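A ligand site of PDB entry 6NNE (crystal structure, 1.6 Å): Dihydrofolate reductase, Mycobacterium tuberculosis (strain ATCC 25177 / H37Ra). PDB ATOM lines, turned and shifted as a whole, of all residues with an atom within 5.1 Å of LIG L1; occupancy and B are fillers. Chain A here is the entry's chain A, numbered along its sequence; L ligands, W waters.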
ATOM      1  N   ILE A   5       8.799  25.641 -15.840  1.00  0.00           N
ATOM      2  CA  ILE A   5       8.703  26.932 -15.166  1.00  0.00           C
ATOM      3  C   ILE A   5       8.611  28.017 -16.249  1.00  0.00           C
ATOM      4  O   ILE A   5       9.403  28.014 -17.206  1.00  0.00           O
ATOM      5  CB  ILE A   5       9.889  27.156 -14.194  1.00  0.00           C
ATOM      6  CG1 ILE A   5       9.737  28.490 -13.442  1.00  0.00           C
ATOM      7  CG2 ILE A   5      11.267  26.983 -14.889  1.00  0.00           C
ATOM      8  CD1 ILE A   5      10.617  28.538 -12.180  1.00  0.00           C
ATOM      9  N   TRP A   6       7.627  28.902 -16.122  1.00  0.00           N
ATOM     10  CA  TRP A   6       7.444  30.008 -17.058  1.00  0.00           C
ATOM     11  C   TRP A   6       6.668  31.134 -16.415  1.00  0.00           C
ATOM     12  O   TRP A   6       6.014  30.980 -15.387  1.00  0.00           O
ATOM     13  CB  TRP A   6       6.735  29.547 -18.339  1.00  0.00           C
ATOM     14  CG  TRP A   6       5.242  29.286 -18.248  1.00  0.00           C
ATOM     15  CD1 TRP A   6       4.230  30.217 -18.323  1.00  0.00           C
ATOM     16  CD2 TRP A   6       4.587  28.007 -18.070  1.00  0.00           C
ATOM     17  NE1 TRP A   6       3.002  29.588 -18.206  1.00  0.00           N
ATOM     18  CE2 TRP A   6       3.197  28.241 -18.063  1.00  0.00           C
ATOM     19  CE3 TRP A   6       5.060  26.699 -17.948  1.00  0.00           C
ATOM     20  CZ2 TRP A   6       2.269  27.205 -17.912  1.00  0.00           C
ATOM     21  CZ3 TRP A   6       4.132  25.664 -17.797  1.00  0.00           C
ATOM     22  CH2 TRP A   6       2.750  25.936 -17.780  1.00  0.00           C
ATOM     23  N   ALA A   7       6.720  32.296 -17.074  1.00  0.00           N
ATOM     24  CA  ALA A   7       5.858  33.430 -16.734  1.00  0.00           C
ATOM     25  C   ALA A   7       4.990  33.765 -17.946  1.00  0.00           C
ATOM     26  O   ALA A   7       5.450  33.668 -19.088  1.00  0.00           O
ATOM     27  CB  ALA A   7       6.687  34.657 -16.328  1.00  0.00           C
ATOM     28  N   GLN A   8       3.741  34.144 -17.704  1.00  0.00           N
ATOM     29  CA  GLN A   8       2.818  34.428 -18.800  1.00  0.00           C
ATOM     30  C   GLN A   8       1.953  35.631 -18.483  1.00  0.00           C
ATOM     31  O   GLN A   8       1.643  35.906 -17.326  1.00  0.00           O
ATOM     32  CB  GLN A   8       1.903  33.219 -19.091  1.00  0.00           C
ATOM     33  CG  GLN A   8       0.926  32.916 -17.952  1.00  0.00           C
ATOM     34  CD  GLN A   8      -0.045  31.811 -18.325  1.00  0.00           C
ATOM     35  OE1 GLN A   8       0.340  30.627 -18.340  1.00  0.00           O
ATOM     36  NE2 GLN A   8      -1.280  32.187 -18.656  1.00  0.00           N
ATOM     37  N   ILE A  14       3.756  34.119 -23.701  1.00  0.00           N
ATOM     38  CA  ILE A  14       5.022  34.048 -22.980  1.00  0.00           C
ATOM     39  C   ILE A  14       6.169  34.750 -23.704  1.00  0.00           C
ATOM     40  O   ILE A  14       7.207  35.006 -23.086  1.00  0.00           O
ATOM     41  CB  ILE A  14       5.428  32.595 -22.653  1.00  0.00           C
ATOM     42  CG1 ILE A  14       5.697  31.779 -23.920  1.00  0.00           C
ATOM     43  CG2 ILE A  14       4.361  31.923 -21.813  1.00  0.00           C
ATOM     44  CD1 ILE A  14       6.496  30.510 -23.679  1.00  0.00           C
ATOM     45  N   GLY A  15       6.037  35.037 -24.998  1.00  0.00           N
ATOM     46  CA  GLY A  15       7.158  35.581 -25.741  1.00  0.00           C
ATOM     47  C   GLY A  15       6.694  36.182 -27.049  1.00  0.00           C
ATOM     48  O   GLY A  15       5.655  35.781 -27.592  1.00  0.00           O
ATOM     49  N   ARG A  16       7.452  37.152 -27.526  1.00  0.00           N
ATOM     50  CA  ARG A  16       7.125  37.912 -28.729  1.00  0.00           C
ATOM     51  C   ARG A  16       8.426  38.390 -29.339  1.00  0.00           C
ATOM     52  O   ARG A  16       9.256  38.964 -28.629  1.00  0.00           O
ATOM     53  CB  ARG A  16       6.211  39.078 -28.356  1.00  0.00           C
ATOM     54  CG  ARG A  16       5.868  40.009 -29.481  1.00  0.00           C
ATOM     55  CD  ARG A  16       4.742  40.910 -29.026  1.00  0.00           C
ATOM     56  NE  ARG A  16       3.509  40.174 -28.813  1.00  0.00           N
ATOM     57  CZ  ARG A  16       2.383  40.712 -28.331  1.00  0.00           C
ATOM     58  NH1 ARG A  16       2.355  41.998 -28.016  1.00  0.00           N
ATOM     59  NH2 ARG A  16       1.296  39.977 -28.180  1.00  0.00           N
ATOM     60  N   GLY A  17       8.623  38.149 -30.633  1.00  0.00           N
ATOM     61  CA  GLY A  17       9.842  38.603 -31.295  1.00  0.00           C
ATOM     62  C   GLY A  17      11.124  37.987 -30.793  1.00  0.00           C
ATOM     63  O   GLY A  17      12.191  38.578 -30.938  1.00  0.00           O
ATOM     64  N   GLY A  18      11.052  36.801 -30.190  1.00  0.00           N
ATOM     65  CA  GLY A  18      12.223  36.153 -29.647  1.00  0.00           C
ATOM     66  C   GLY A  18      12.613  36.565 -28.239  1.00  0.00           C
ATOM     67  O   GLY A  18      13.629  36.085 -27.753  1.00  0.00           O
ATOM     68  N   ASP A  19      11.830  37.430 -27.593  1.00  0.00           N
ATOM     69  CA  ASP A  19      12.140  37.891 -26.239  1.00  0.00           C
ATOM     70  C   ASP A  19      10.848  37.939 -25.438  1.00  0.00           C
ATOM     71  O   ASP A  19       9.849  37.333 -25.821  1.00  0.00           O
ATOM     72  CB  ASP A  19      12.864  39.251 -26.286  1.00  0.00           C
ATOM     73  CG  ASP A  19      13.836  39.409 -25.149  1.00  0.00           C
ATOM     74  OD1 ASP A  19      15.041  39.109 -25.346  1.00  0.00           O
ATOM     75  OD2 ASP A  19      13.387  39.815 -24.039  1.00  0.00           O
ATOM     76  N   ILE A  20      10.890  38.616 -24.295  1.00  0.00           N
ATOM     77  CA  ILE A  20       9.785  38.633 -23.341  1.00  0.00           C
ATOM     78  C   ILE A  20       9.394  40.092 -23.128  1.00  0.00           C
ATOM     79  O   ILE A  20      10.269  40.920 -22.873  1.00  0.00           O
ATOM     80  CB  ILE A  20      10.174  37.974 -22.001  1.00  0.00           C
ATOM     81  CG1 ILE A  20      10.688  36.555 -22.254  1.00  0.00           C
ATOM     82  CG2 ILE A  20       8.972  37.954 -21.038  1.00  0.00           C
ATOM     83  CD1 ILE A  20      11.321  35.881 -21.063  1.00  0.00           C
ATOM     84  N   TRP A  22       8.262  41.875 -20.735  1.00  0.00           N
ATOM     85  CA  TRP A  22       8.255  42.375 -19.355  1.00  0.00           C
ATOM     86  C   TRP A  22       9.520  41.858 -18.691  1.00  0.00           C
ATOM     87  O   TRP A  22      10.238  41.035 -19.248  1.00  0.00           O
ATOM     88  CB  TRP A  22       6.999  41.932 -18.584  1.00  0.00           C
ATOM     89  CG  TRP A  22       6.932  40.419 -18.474  1.00  0.00           C
ATOM     90  CD1 TRP A  22       7.658  39.619 -17.635  1.00  0.00           C
ATOM     91  CD2 TRP A  22       6.120  39.549 -19.264  1.00  0.00           C
ATOM     92  NE1 TRP A  22       7.345  38.297 -17.859  1.00  0.00           N
ATOM     93  CE2 TRP A  22       6.394  38.234 -18.848  1.00  0.00           C
ATOM     94  CE3 TRP A  22       5.165  39.754 -20.275  1.00  0.00           C
ATOM     95  CZ2 TRP A  22       5.765  37.118 -19.417  1.00  0.00           C
ATOM     96  CZ3 TRP A  22       4.549  38.644 -20.834  1.00  0.00           C
ATOM     97  CH2 TRP A  22       4.858  37.350 -20.404  1.00  0.00           C
ATOM     98  N   GLY A  43      14.878  25.160 -25.401  1.00  0.00           N
ATOM     99  CA  GLY A  43      15.004  25.177 -26.839  1.00  0.00           C
ATOM    100  C   GLY A  43      16.067  26.143 -27.309  1.00  0.00           C
ATOM    101  O   GLY A  43      16.489  27.052 -26.602  1.00  0.00           O
ATOM    102  N   ARG A  44      16.510  25.927 -28.544  1.00  0.00           N
ATOM    103  CA  ARG A  44      17.624  26.732 -29.072  1.00  0.00           C
ATOM    104  C   ARG A  44      17.261  28.207 -29.148  1.00  0.00           C
ATOM    105  O   ARG A  44      18.098  29.065 -28.903  1.00  0.00           O
ATOM    106  CB  ARG A  44      18.041  26.176 -30.437  1.00  0.00           C
ATOM    107  CG  ARG A  44      19.335  26.781 -31.002  1.00  0.00           C
ATOM    108  CD  ARG A  44      19.065  27.986 -31.936  1.00  0.00           C
ATOM    109  NE  ARG A  44      18.114  27.636 -32.991  1.00  0.00           N
ATOM    110  CZ  ARG A  44      17.436  28.525 -33.717  1.00  0.00           C
ATOM    111  NH1 ARG A  44      17.612  29.821 -33.500  1.00  0.00           N
ATOM    112  NH2 ARG A  44      16.591  28.106 -34.655  1.00  0.00           N
ATOM    113  N   ARG A  45      16.014  28.528 -29.503  1.00  0.00           N
ATOM    114  CA  ARG A  45      15.635  29.937 -29.553  1.00  0.00           C
ATOM    115  C   ARG A  45      15.713  30.601 -28.178  1.00  0.00           C
ATOM    116  O   ARG A  45      16.082  31.775 -28.071  1.00  0.00           O
ATOM    117  CB  ARG A  45      14.242  30.071 -30.143  1.00  0.00           C
ATOM    118  CG  ARG A  45      14.150  29.676 -31.622  1.00  0.00           C
ATOM    119  CD  ARG A  45      12.760  30.023 -32.104  1.00  0.00           C
ATOM    120  NE  ARG A  45      12.570  29.822 -33.533  1.00  0.00           N
ATOM    121  CZ  ARG A  45      11.367  29.705 -34.092  1.00  0.00           C
ATOM    122  NH1 ARG A  45      10.275  29.757 -33.326  1.00  0.00           N
ATOM    123  NH2 ARG A  45      11.258  29.530 -35.396  1.00  0.00           N
ATOM    124  N   THR A  46      15.364  29.863 -27.122  1.00  0.00           N
ATOM    125  CA  THR A  46      15.485  30.420 -25.769  1.00  0.00           C
ATOM    126  C   THR A  46      16.945  30.614 -25.366  1.00  0.00           C
ATOM    127  O   THR A  46      17.300  31.631 -24.750  1.00  0.00           O
ATOM    128  CB  THR A  46      14.737  29.517 -24.777  1.00  0.00           C
ATOM    129  OG1 THR A  46      13.328  29.621 -25.031  1.00  0.00           O
ATOM    130  CG2 THR A  46      14.975  29.969 -23.337  1.00  0.00           C
ATOM    131  N   SER A  49      18.000  33.718 -26.750  1.00  0.00           N
ATOM    132  CA  SER A  49      17.450  34.872 -26.045  1.00  0.00           C
ATOM    133  C   SER A  49      18.242  35.245 -24.805  1.00  0.00           C
ATOM    134  O   SER A  49      17.989  36.305 -24.222  1.00  0.00           O
ATOM    135  CB  SER A  49      15.988  34.597 -25.670  1.00  0.00           C
ATOM    136  OG  SER A  49      15.887  33.885 -24.440  1.00  0.00           O
ATOM    137  N   LEU A  65      18.165  22.047 -26.608  1.00  0.00           N
ATOM    138  CA  LEU A  65      17.579  21.173 -27.625  1.00  0.00           C
ATOM    139  C   LEU A  65      17.633  21.825 -29.002  1.00  0.00           C
ATOM    140  O   LEU A  65      17.192  22.969 -29.160  1.00  0.00           O
ATOM    141  CB  LEU A  65      16.133  20.863 -27.250  1.00  0.00           C
ATOM    142  CG  LEU A  65      15.340  19.828 -28.023  1.00  0.00           C
ATOM    143  CD1 LEU A  65      15.925  18.445 -27.806  1.00  0.00           C
ATOM    144  CD2 LEU A  65      13.907  19.879 -27.553  1.00  0.00           C
ATOM    145  N   SER A  66      18.207  21.112 -29.975  1.00  0.00           N
ATOM    146  CA  SER A  66      18.330  21.602 -31.338  1.00  0.00           C
ATOM    147  C   SER A  66      18.350  20.411 -32.270  1.00  0.00           C
ATOM    148  O   SER A  66      18.886  19.351 -31.931  1.00  0.00           O
ATOM    149  CB  SER A  66      19.610  22.441 -31.538  1.00  0.00           C
ATOM    150  OG  SER A  66      19.770  22.889 -32.885  1.00  0.00           O
ATOM    151  N   ARG A  67      17.768  20.593 -33.452  1.00  0.00           N
ATOM    152  CA  ARG A  67      17.893  19.604 -34.515  1.00  0.00           C
ATOM    153  C   ARG A  67      19.155  19.789 -35.345  1.00  0.00           C
ATOM    154  O   ARG A  67      19.427  18.958 -36.221  1.00  0.00           O
ATOM    155  CB  ARG A  67      16.661  19.644 -35.423  1.00  0.00           C
ATOM    156  CG  ARG A  67      15.374  19.195 -34.735  1.00  0.00           C
ATOM    157  CD  ARG A  67      14.211  19.075 -35.722  1.00  0.00           C
ATOM    158  NE  ARG A  67      12.930  18.819 -35.055  1.00  0.00           N
ATOM    159  CZ  ARG A  67      12.129  19.772 -34.581  1.00  0.00           C
ATOM    160  NH1 ARG A  67      12.487  21.044 -34.686  1.00  0.00           N
ATOM    161  NH2 ARG A  67      10.989  19.440 -33.998  1.00  0.00           N
ATOM    162  N   GLN A  68      19.929  20.847 -35.103  1.00  0.00           N
ATOM    163  CA  GLN A  68      21.160  21.098 -35.840  1.00  0.00           C
ATOM    164  C   GLN A  68      22.278  20.289 -35.201  1.00  0.00           C
ATOM    165  O   GLN A  68      22.688  20.568 -34.069  1.00  0.00           O
ATOM    166  CB  GLN A  68      21.534  22.585 -35.816  1.00  0.00           C
ATOM    167  CG  GLN A  68      20.524  23.560 -36.358  1.00  0.00           C
ATOM    168  CD  GLN A  68      20.987  25.002 -36.134  1.00  0.00           C
ATOM    169  OE1 GLN A  68      22.117  25.363 -36.491  1.00  0.00           O
ATOM    170  NE2 GLN A  68      20.110  25.822 -35.534  1.00  0.00           N
ATOM    171  N   GLY A  80      19.815  16.347 -29.392  1.00  0.00           N
ATOM    172  CA  GLY A  80      18.843  16.290 -30.472  1.00  0.00           C
ATOM    173  C   GLY A  80      17.463  15.798 -30.088  1.00  0.00           C
ATOM    174  O   GLY A  80      16.552  15.815 -30.924  1.00  0.00           O
ATOM    175  N   SER A  81      17.291  15.360 -28.852  1.00  0.00           N
ATOM    176  CA  SER A  81      16.015  14.866 -28.363  1.00  0.00           C
ATOM    177  C   SER A  81      15.899  15.159 -26.874  1.00  0.00           C
ATOM    178  O   SER A  81      16.909  15.294 -26.171  1.00  0.00           O
ATOM    179  CB  SER A  81      15.865  13.356 -28.619  1.00  0.00           C
ATOM    180  OG  SER A  81      16.659  12.618 -27.706  1.00  0.00           O
ATOM    181  N   ILE A  94      12.873  25.264 -19.109  1.00  0.00           N
ATOM    182  CA  ILE A  94      12.817  26.702 -18.877  1.00  0.00           C
ATOM    183  C   ILE A  94      12.437  27.484 -20.133  1.00  0.00           C
ATOM    184  O   ILE A  94      12.564  28.713 -20.157  1.00  0.00           O
ATOM    185  CB  ILE A  94      14.144  27.232 -18.302  1.00  0.00           C
ATOM    186  CG1 ILE A  94      15.282  27.141 -19.320  1.00  0.00           C
ATOM    187  CG2 ILE A  94      14.536  26.443 -17.028  1.00  0.00           C
ATOM    188  CD1 ILE A  94      16.446  28.105 -19.020  1.00  0.00           C
ATOM    189  N   GLY A  95      11.940  26.808 -21.166  1.00  0.00           N
ATOM    190  CA  GLY A  95      11.416  27.464 -22.361  1.00  0.00           C
ATOM    191  C   GLY A  95      11.970  26.859 -23.626  1.00  0.00           C
ATOM    192  O   GLY A  95      12.866  26.016 -23.611  1.00  0.00           O
ATOM    193  N   GLY A  96      11.375  27.261 -24.758  1.00  0.00           N
ATOM    194  CA  GLY A  96      10.259  28.197 -24.866  1.00  0.00           C
ATOM    195  C   GLY A  96       8.952  27.495 -25.229  1.00  0.00           C
ATOM    196  O   GLY A  96       8.710  26.388 -24.779  1.00  0.00           O
ATOM    197  N   GLY A  97       8.097  28.141 -26.027  1.00  0.00           N
ATOM    198  CA  GLY A  97       6.782  27.569 -26.282  1.00  0.00           C
ATOM    199  C   GLY A  97       6.812  26.175 -26.874  1.00  0.00           C
ATOM    200  O   GLY A  97       6.039  25.301 -26.475  1.00  0.00           O
ATOM    201  N   GLN A  98       7.701  25.950 -27.846  1.00  0.00           N
ATOM    202  CA  GLN A  98       7.801  24.648 -28.482  1.00  0.00           C
ATOM    203  C   GLN A  98       8.240  23.576 -27.485  1.00  0.00           C
ATOM    204  O   GLN A  98       7.684  22.476 -27.464  1.00  0.00           O
ATOM    205  CB  GLN A  98       8.788  24.695 -29.648  1.00  0.00           C
ATOM    206  CG  GLN A  98       8.274  25.426 -30.855  1.00  0.00           C
ATOM    207  CD  GLN A  98       9.263  25.406 -32.008  1.00  0.00           C
ATOM    208  OE1 GLN A  98      10.121  24.523 -32.095  1.00  0.00           O
ATOM    209  NE2 GLN A  98       9.175  26.405 -32.877  1.00  0.00           N
ATOM    210  N   VAL A  99       9.256  23.884 -26.684  1.00  0.00           N
ATOM    211  CA  VAL A  99       9.792  22.863 -25.795  1.00  0.00           C
ATOM    212  C   VAL A  99       8.846  22.607 -24.615  1.00  0.00           C
ATOM    213  O   VAL A  99       8.743  21.462 -24.154  1.00  0.00           O
ATOM    214  CB  VAL A  99      11.220  23.234 -25.364  1.00  0.00           C
ATOM    215  CG1 VAL A  99      11.771  22.209 -24.342  1.00  0.00           C
ATOM    216  CG2 VAL A  99      12.126  23.259 -26.592  1.00  0.00           C
ATOM    217  N   TYR A 100       8.105  23.623 -24.139  1.00  0.00           N
ATOM    218  CA  TYR A 100       7.087  23.348 -23.125  1.00  0.00           C
ATOM    219  C   TYR A 100       6.073  22.340 -23.645  1.00  0.00           C
ATOM    220  O   TYR A 100       5.684  21.401 -22.930  1.00  0.00           O
ATOM    221  CB  TYR A 100       6.327  24.619 -22.694  1.00  0.00           C
ATOM    222  CG  TYR A 100       7.138  25.629 -21.918  1.00  0.00           C
ATOM    223  CD1 TYR A 100       7.960  25.235 -20.853  1.00  0.00           C
ATOM    224  CD2 TYR A 100       7.072  26.967 -22.241  1.00  0.00           C
ATOM    225  CE1 TYR A 100       8.700  26.173 -20.153  1.00  0.00           C
ATOM    226  CE2 TYR A 100       7.810  27.898 -21.553  1.00  0.00           C
ATOM    227  CZ  TYR A 100       8.609  27.503 -20.508  1.00  0.00           C
ATOM    228  OH  TYR A 100       9.338  28.447 -19.826  1.00  0.00           O
ATOM    229  N   LEU A 102       6.513  20.102 -25.990  1.00  0.00           N
ATOM    230  CA  LEU A 102       7.191  18.819 -26.148  1.00  0.00           C
ATOM    231  C   LEU A 102       7.379  18.111 -24.805  1.00  0.00           C
ATOM    232  O   LEU A 102       7.319  16.880 -24.734  1.00  0.00           O
ATOM    233  CB  LEU A 102       8.550  19.051 -26.817  1.00  0.00           C
ATOM    234  CG  LEU A 102       9.415  17.845 -27.125  1.00  0.00           C
ATOM    235  CD1 LEU A 102       8.828  17.069 -28.281  1.00  0.00           C
ATOM    236  CD2 LEU A 102      10.805  18.303 -27.466  1.00  0.00           C
ATOM    237  N   ALA A 126       4.841  33.242 -28.817  1.00  0.00           N
ATOM    238  CA  ALA A 126       4.972  31.975 -28.118  1.00  0.00           C
ATOM    239  C   ALA A 126       3.954  31.964 -26.991  1.00  0.00           C
ATOM    240  O   ALA A 126       3.712  32.987 -26.356  1.00  0.00           O
ATOM    241  CB  ALA A 126       6.393  31.797 -27.583  1.00  0.00           C
HETATM  242  P1  LIG L   1      12.031  27.407 -28.239  1.00  0.00           P
HETATM  243  O1  LIG L   1      11.036  26.418 -27.769  1.00  0.00           O
HETATM  244  O2  LIG L   1      12.843  28.201 -27.271  1.00  0.00           O
HETATM  245  O3  LIG L   1      13.178  26.702 -29.193  1.00  0.00           O
HETATM  246  C1  LIG L   1      12.601  26.133 -30.347  1.00  0.00           C
HETATM  247  C2  LIG L   1      13.774  25.353 -30.981  1.00  0.00           C
HETATM  248  O4  LIG L   1      14.065  24.189 -30.183  1.00  0.00           O
HETATM  249  C3  LIG L   1      13.518  24.840 -32.416  1.00  0.00           C
HETATM  250  O5  LIG L   1      13.786  25.853 -33.381  1.00  0.00           O
HETATM  251  C4  LIG L   1      14.617  23.722 -32.490  1.00  0.00           C
HETATM  252  O6  LIG L   1      15.866  24.193 -32.495  1.00  0.00           O
HETATM  253  C5  LIG L   1      14.452  23.108 -31.063  1.00  0.00           C
HETATM  254  N1  LIG L   1      13.450  22.072 -31.021  1.00  0.00           N
HETATM  255  C6  LIG L   1      12.058  22.193 -30.898  1.00  0.00           C
HETATM  256  N2  LIG L   1      11.433  20.983 -30.891  1.00  0.00           N
HETATM  257  C7  LIG L   1      12.484  20.066 -31.022  1.00  0.00           C
HETATM  258  C8  LIG L   1      12.503  18.656 -31.089  1.00  0.00           C
HETATM  259  N3  LIG L   1      11.344  17.924 -31.026  1.00  0.00           N
HETATM  260  N4  LIG L   1      13.673  17.987 -31.205  1.00  0.00           N
HETATM  261  C9  LIG L   1      14.807  18.766 -31.274  1.00  0.00           C
HETATM  262  N5  LIG L   1      14.937  20.103 -31.229  1.00  0.00           N
HETATM  263  C10 LIG L   1      13.742  20.734 -31.111  1.00  0.00           C
HETATM  264  O7  LIG L   1      11.298  28.403 -29.388  1.00  0.00           O
HETATM  265  P2  LIG L   1       9.913  29.202 -29.179  1.00  0.00           P
HETATM  266  O8  LIG L   1       9.973  30.209 -30.265  1.00  0.00           O
HETATM  267  O9  LIG L   1       8.695  28.332 -29.023  1.00  0.00           O
HETATM  268  O10 LIG L   1       9.986  30.016 -27.691  1.00  0.00           O
HETATM  269  C11 LIG L   1      10.868  31.122 -27.715  1.00  0.00           C
HETATM  270  C12 LIG L   1      10.125  32.280 -27.015  1.00  0.00           C
HETATM  271  O11 LIG L   1       9.808  31.912 -25.624  1.00  0.00           O
HETATM  272  C13 LIG L   1      11.011  33.537 -26.937  1.00  0.00           C
HETATM  273  O12 LIG L   1      10.184  34.672 -27.160  1.00  0.00           O
HETATM  274  C14 LIG L   1      11.475  33.502 -25.467  1.00  0.00           C
HETATM  275  O13 LIG L   1      11.783  34.776 -24.965  1.00  0.00           O
HETATM  276  C15 LIG L   1      10.167  33.003 -24.811  1.00  0.00           C
HETATM  277  N6  LIG L   1      10.371  32.514 -23.432  1.00  0.00           N
HETATM  278  C16 LIG L   1       9.539  32.962 -22.426  1.00  0.00           C
HETATM  279  C17 LIG L   1       9.711  32.546 -21.150  1.00  0.00           C
HETATM  280  C18 LIG L   1       8.817  33.056 -20.143  1.00  0.00           C
HETATM  281  O14 LIG L   1       8.844  32.642 -18.978  1.00  0.00           O
HETATM  282  N7  LIG L   1       7.942  34.075 -20.455  1.00  0.00           N
HETATM  283  C19 LIG L   1      10.782  31.603 -20.739  1.00  0.00           C
HETATM  284  C20 LIG L   1      11.616  31.151 -21.892  1.00  0.00           C
HETATM  285  C21 LIG L   1      11.410  31.586 -23.140  1.00  0.00           C
HETATM  286  P3  LIG L   1      16.728  24.318 -34.047  1.00  0.00           P
HETATM  287  O15 LIG L   1      15.867  25.327 -34.747  1.00  0.00           O
HETATM  288  O16 LIG L   1      18.105  24.838 -33.633  1.00  0.00           O
HETATM  289  O17 LIG L   1      16.665  22.905 -34.543  1.00  0.00           O
HETATM  290  N1  LG2 L   2       9.315  32.372 -14.427  1.00  0.00           N
HETATM  291  C1  LG2 L   2      16.354  34.565 -17.850  1.00  0.00           C
HETATM  292  C2  LG2 L   2      16.073  37.907 -18.867  1.00  0.00           C
HETATM  293  O1  LG2 L   2      16.761  36.680 -18.927  1.00  0.00           O
HETATM  294  C3  LG2 L   2      15.948  35.532 -18.784  1.00  0.00           C
HETATM  295  C4  LG2 L   2      14.778  35.325 -19.546  1.00  0.00           C
HETATM  296  C5  LG2 L   2      14.030  34.162 -19.350  1.00  0.00           C
HETATM  297  C6  LG2 L   2      14.438  33.190 -18.396  1.00  0.00           C
HETATM  298  C7  LG2 L   2      13.604  31.915 -18.192  1.00  0.00           C
HETATM  299  C8  LG2 L   2      12.462  32.109 -17.167  1.00  0.00           C
HETATM  300  C9  LG2 L   2      12.258  33.293 -16.409  1.00  0.00           C
HETATM  301  N2  LG2 L   2      11.210  33.336 -15.515  1.00  0.00           N
HETATM  302  C10 LG2 L   2      10.393  32.290 -15.355  1.00  0.00           C
HETATM  303  N3  LG2 L   2      10.549  31.139 -16.048  1.00  0.00           N
HETATM  304  C11 LG2 L   2      11.533  31.015 -16.949  1.00  0.00           C
HETATM  305  N4  LG2 L   2      11.641  29.776 -17.672  1.00  0.00           N
HETATM  306  C12 LG2 L   2      15.595  33.392 -17.646  1.00  0.00           C
HETATM  307  O2  LG2 L   2      17.559  34.838 -17.126  1.00  0.00           O
HETATM  308  C13 LG2 L   2      17.902  33.822 -16.158  1.00  0.00           C
HETATM  309  O   HOH W   1       8.816  20.275 -31.225  1.00  0.00           O
HETATM  310  O   HOH W   2      15.684  25.821 -37.403  1.00  0.00           O
HETATM  311  O   HOH W   3       9.753  32.717 -30.678  1.00  0.00           O
HETATM  312  O   HOH W   4       9.641  35.728 -17.627  1.00  0.00           O
HETATM  313  O   HOH W   5      10.429  14.890 -31.544  1.00  0.00           O
HETATM  314  O   HOH W   6       8.836  34.994 -29.561  1.00  0.00           O
HETATM  315  O   HOH W   7      13.704  34.652 -23.127  1.00  0.00           O
HETATM  316  O   HOH W   8      14.511  22.392 -36.013  1.00  0.00           O
HETATM  317  O   HOH W   9       6.439  28.980 -30.134  1.00  0.00           O
HETATM  318  O   HOH W  10      12.564  24.497 -35.815  1.00  0.00           O
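O of Ile 14 lies within hydrogen-bond range of N7 of LIG L1, 2.9 Å away.
The side-chain hydroxyl (OG1) of Thr 46 sits at hydrogen-bond distance from an oxygen (O2) of LIG L1, at 2.7 Å.
The backbone NH (N) of Gly 96 sits at hydrogen-bond distance from an oxygen (O2) of LIG L1 (3.1 Å).
The side-chain amide nitrogen (NE2) of Gln 68 lies within hydrogen-bond range of an oxygen (O16) of LIG L1.
O2 of LIG L1 is in hydrogen-bond range of N of Thr 46, at 3.0 Å.
The backbone carbonyl oxygen (O) of Asp 19 lies within hydrogen-bond range of an oxygen (O12) of LIG L1.
O14 of LIG L1 lies within hydrogen-bond range of N of Ala 7, 2.9 Å away.
The backbone NH (N) of Gly 97 lies within hydrogen-bond range of an oxygen (O9) of LIG L1 (3.1 Å).
The side-chain hydroxyl (OG) of Ser 66 is in hydrogen-bond range of an oxygen (O16) of LIG L1, at 2.7 Å.
The backbone NH (N) of Gln 98 is in hydrogen-bond range of an oxygen (O9) of LIG L1, 2.8 Å away.
The guanidinium group of Arg 44 is in salt-bridge range of an oxygen (O16) of LIG L1 (2.9 Å).
The backbone carbonyl oxygen of Ala 7 sits at hydrogen-bond distance from a nitrogen (N7) of LIG L1 (2.9 Å).
An oxygen (O3) of LIG L1 is in hydrogen-bond range of the backbone NH (N) of Arg 45 (3.4 Å).
N of Arg 44 lies within hydrogen-bond range of O4 of LIG L1 (3.4 Å).
The backbone NH (N) of Arg 67 is in hydrogen-bond range of an oxygen (O17) of LIG L1.
O of Ile 94 lies within hydrogen-bond range of N4 of LG2 L2.
N of Asp 19 sits at hydrogen-bond distance from O12 of LIG L1.
O of Ile 5 is in hydrogen-bond range of N4 of LG2 L2 (2.9 Å).
OH of Tyr 100 is in hydrogen-bond range of N4 of LG2 L2.
A nitrogen (N2) of LIG L1 sits close to the guanidinium group of Arg 67, 3.5 Å away.
NH1 of Arg 45 is in salt-bridge range of O8 of LIG L1 (3.1 Å).
The backbone NH (N) of Val 99 lies within hydrogen-bond range of an oxygen (O1) of LIG L1, at 3.3 Å.
The backbone NH (N) of Ile 14 sits at hydrogen-bond distance from the backbone carbonyl oxygen (O) of Ala 126 (2.9 Å).
The indole nitrogen (NE1) of Trp 6 is in hydrogen-bond range of the side-chain amide oxygen (OE1) of Gln 8.
The side-chain hydroxyl (OG) of Ser 66 is in hydrogen-bond range of the backbone NH (N) of Gln 68.
N of Gly 43 sits at hydrogen-bond distance from O of Gly 95, 2.8 Å away.
OG1 of Thr 46 lies within hydrogen-bond range of N of Gly 96 (3.1 Å).
O of Gly 15 sits at hydrogen-bond distance from N of Ala 126 (2.9 Å).
The side-chain hydroxyl of Ser 49 lies within hydrogen-bond range of the backbone carbonyl oxygen of Thr 46 (2.7 Å).
N of Gly 95 lies within hydrogen-bond range of OH of Tyr 100.
Merely in contact with LIG L1: Trp 6, Gly 15, Arg 16, Gly 18, Ile 20, Trp 22, Gly 43, Leu 65, Gly 80, Ile 94, Gly 95, Tyr 100, Leu 102 and Ala 126.
Hydrophobic or aromatic side chains within 4 Å of LIG L1: Trp 6, Ala 7, Ile 14, Ile 20, Trp 22, Leu 65, Val 99, Leu 102 and Ala 126.
The nearest printed residue that does not touch LIG L1 is Ser 49 (4.2 Å).
Water W8 bridges O17 of LIG L1 (2.7 Å) and NH1 of Arg 67 (2.8 Å).
Water W7 bridges OG of Ser 49 (2.7 Å) and O13 of LIG L1 (2.7 Å).
Water W4 bridges NE1 of Trp 22 and O14 of LIG L1.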
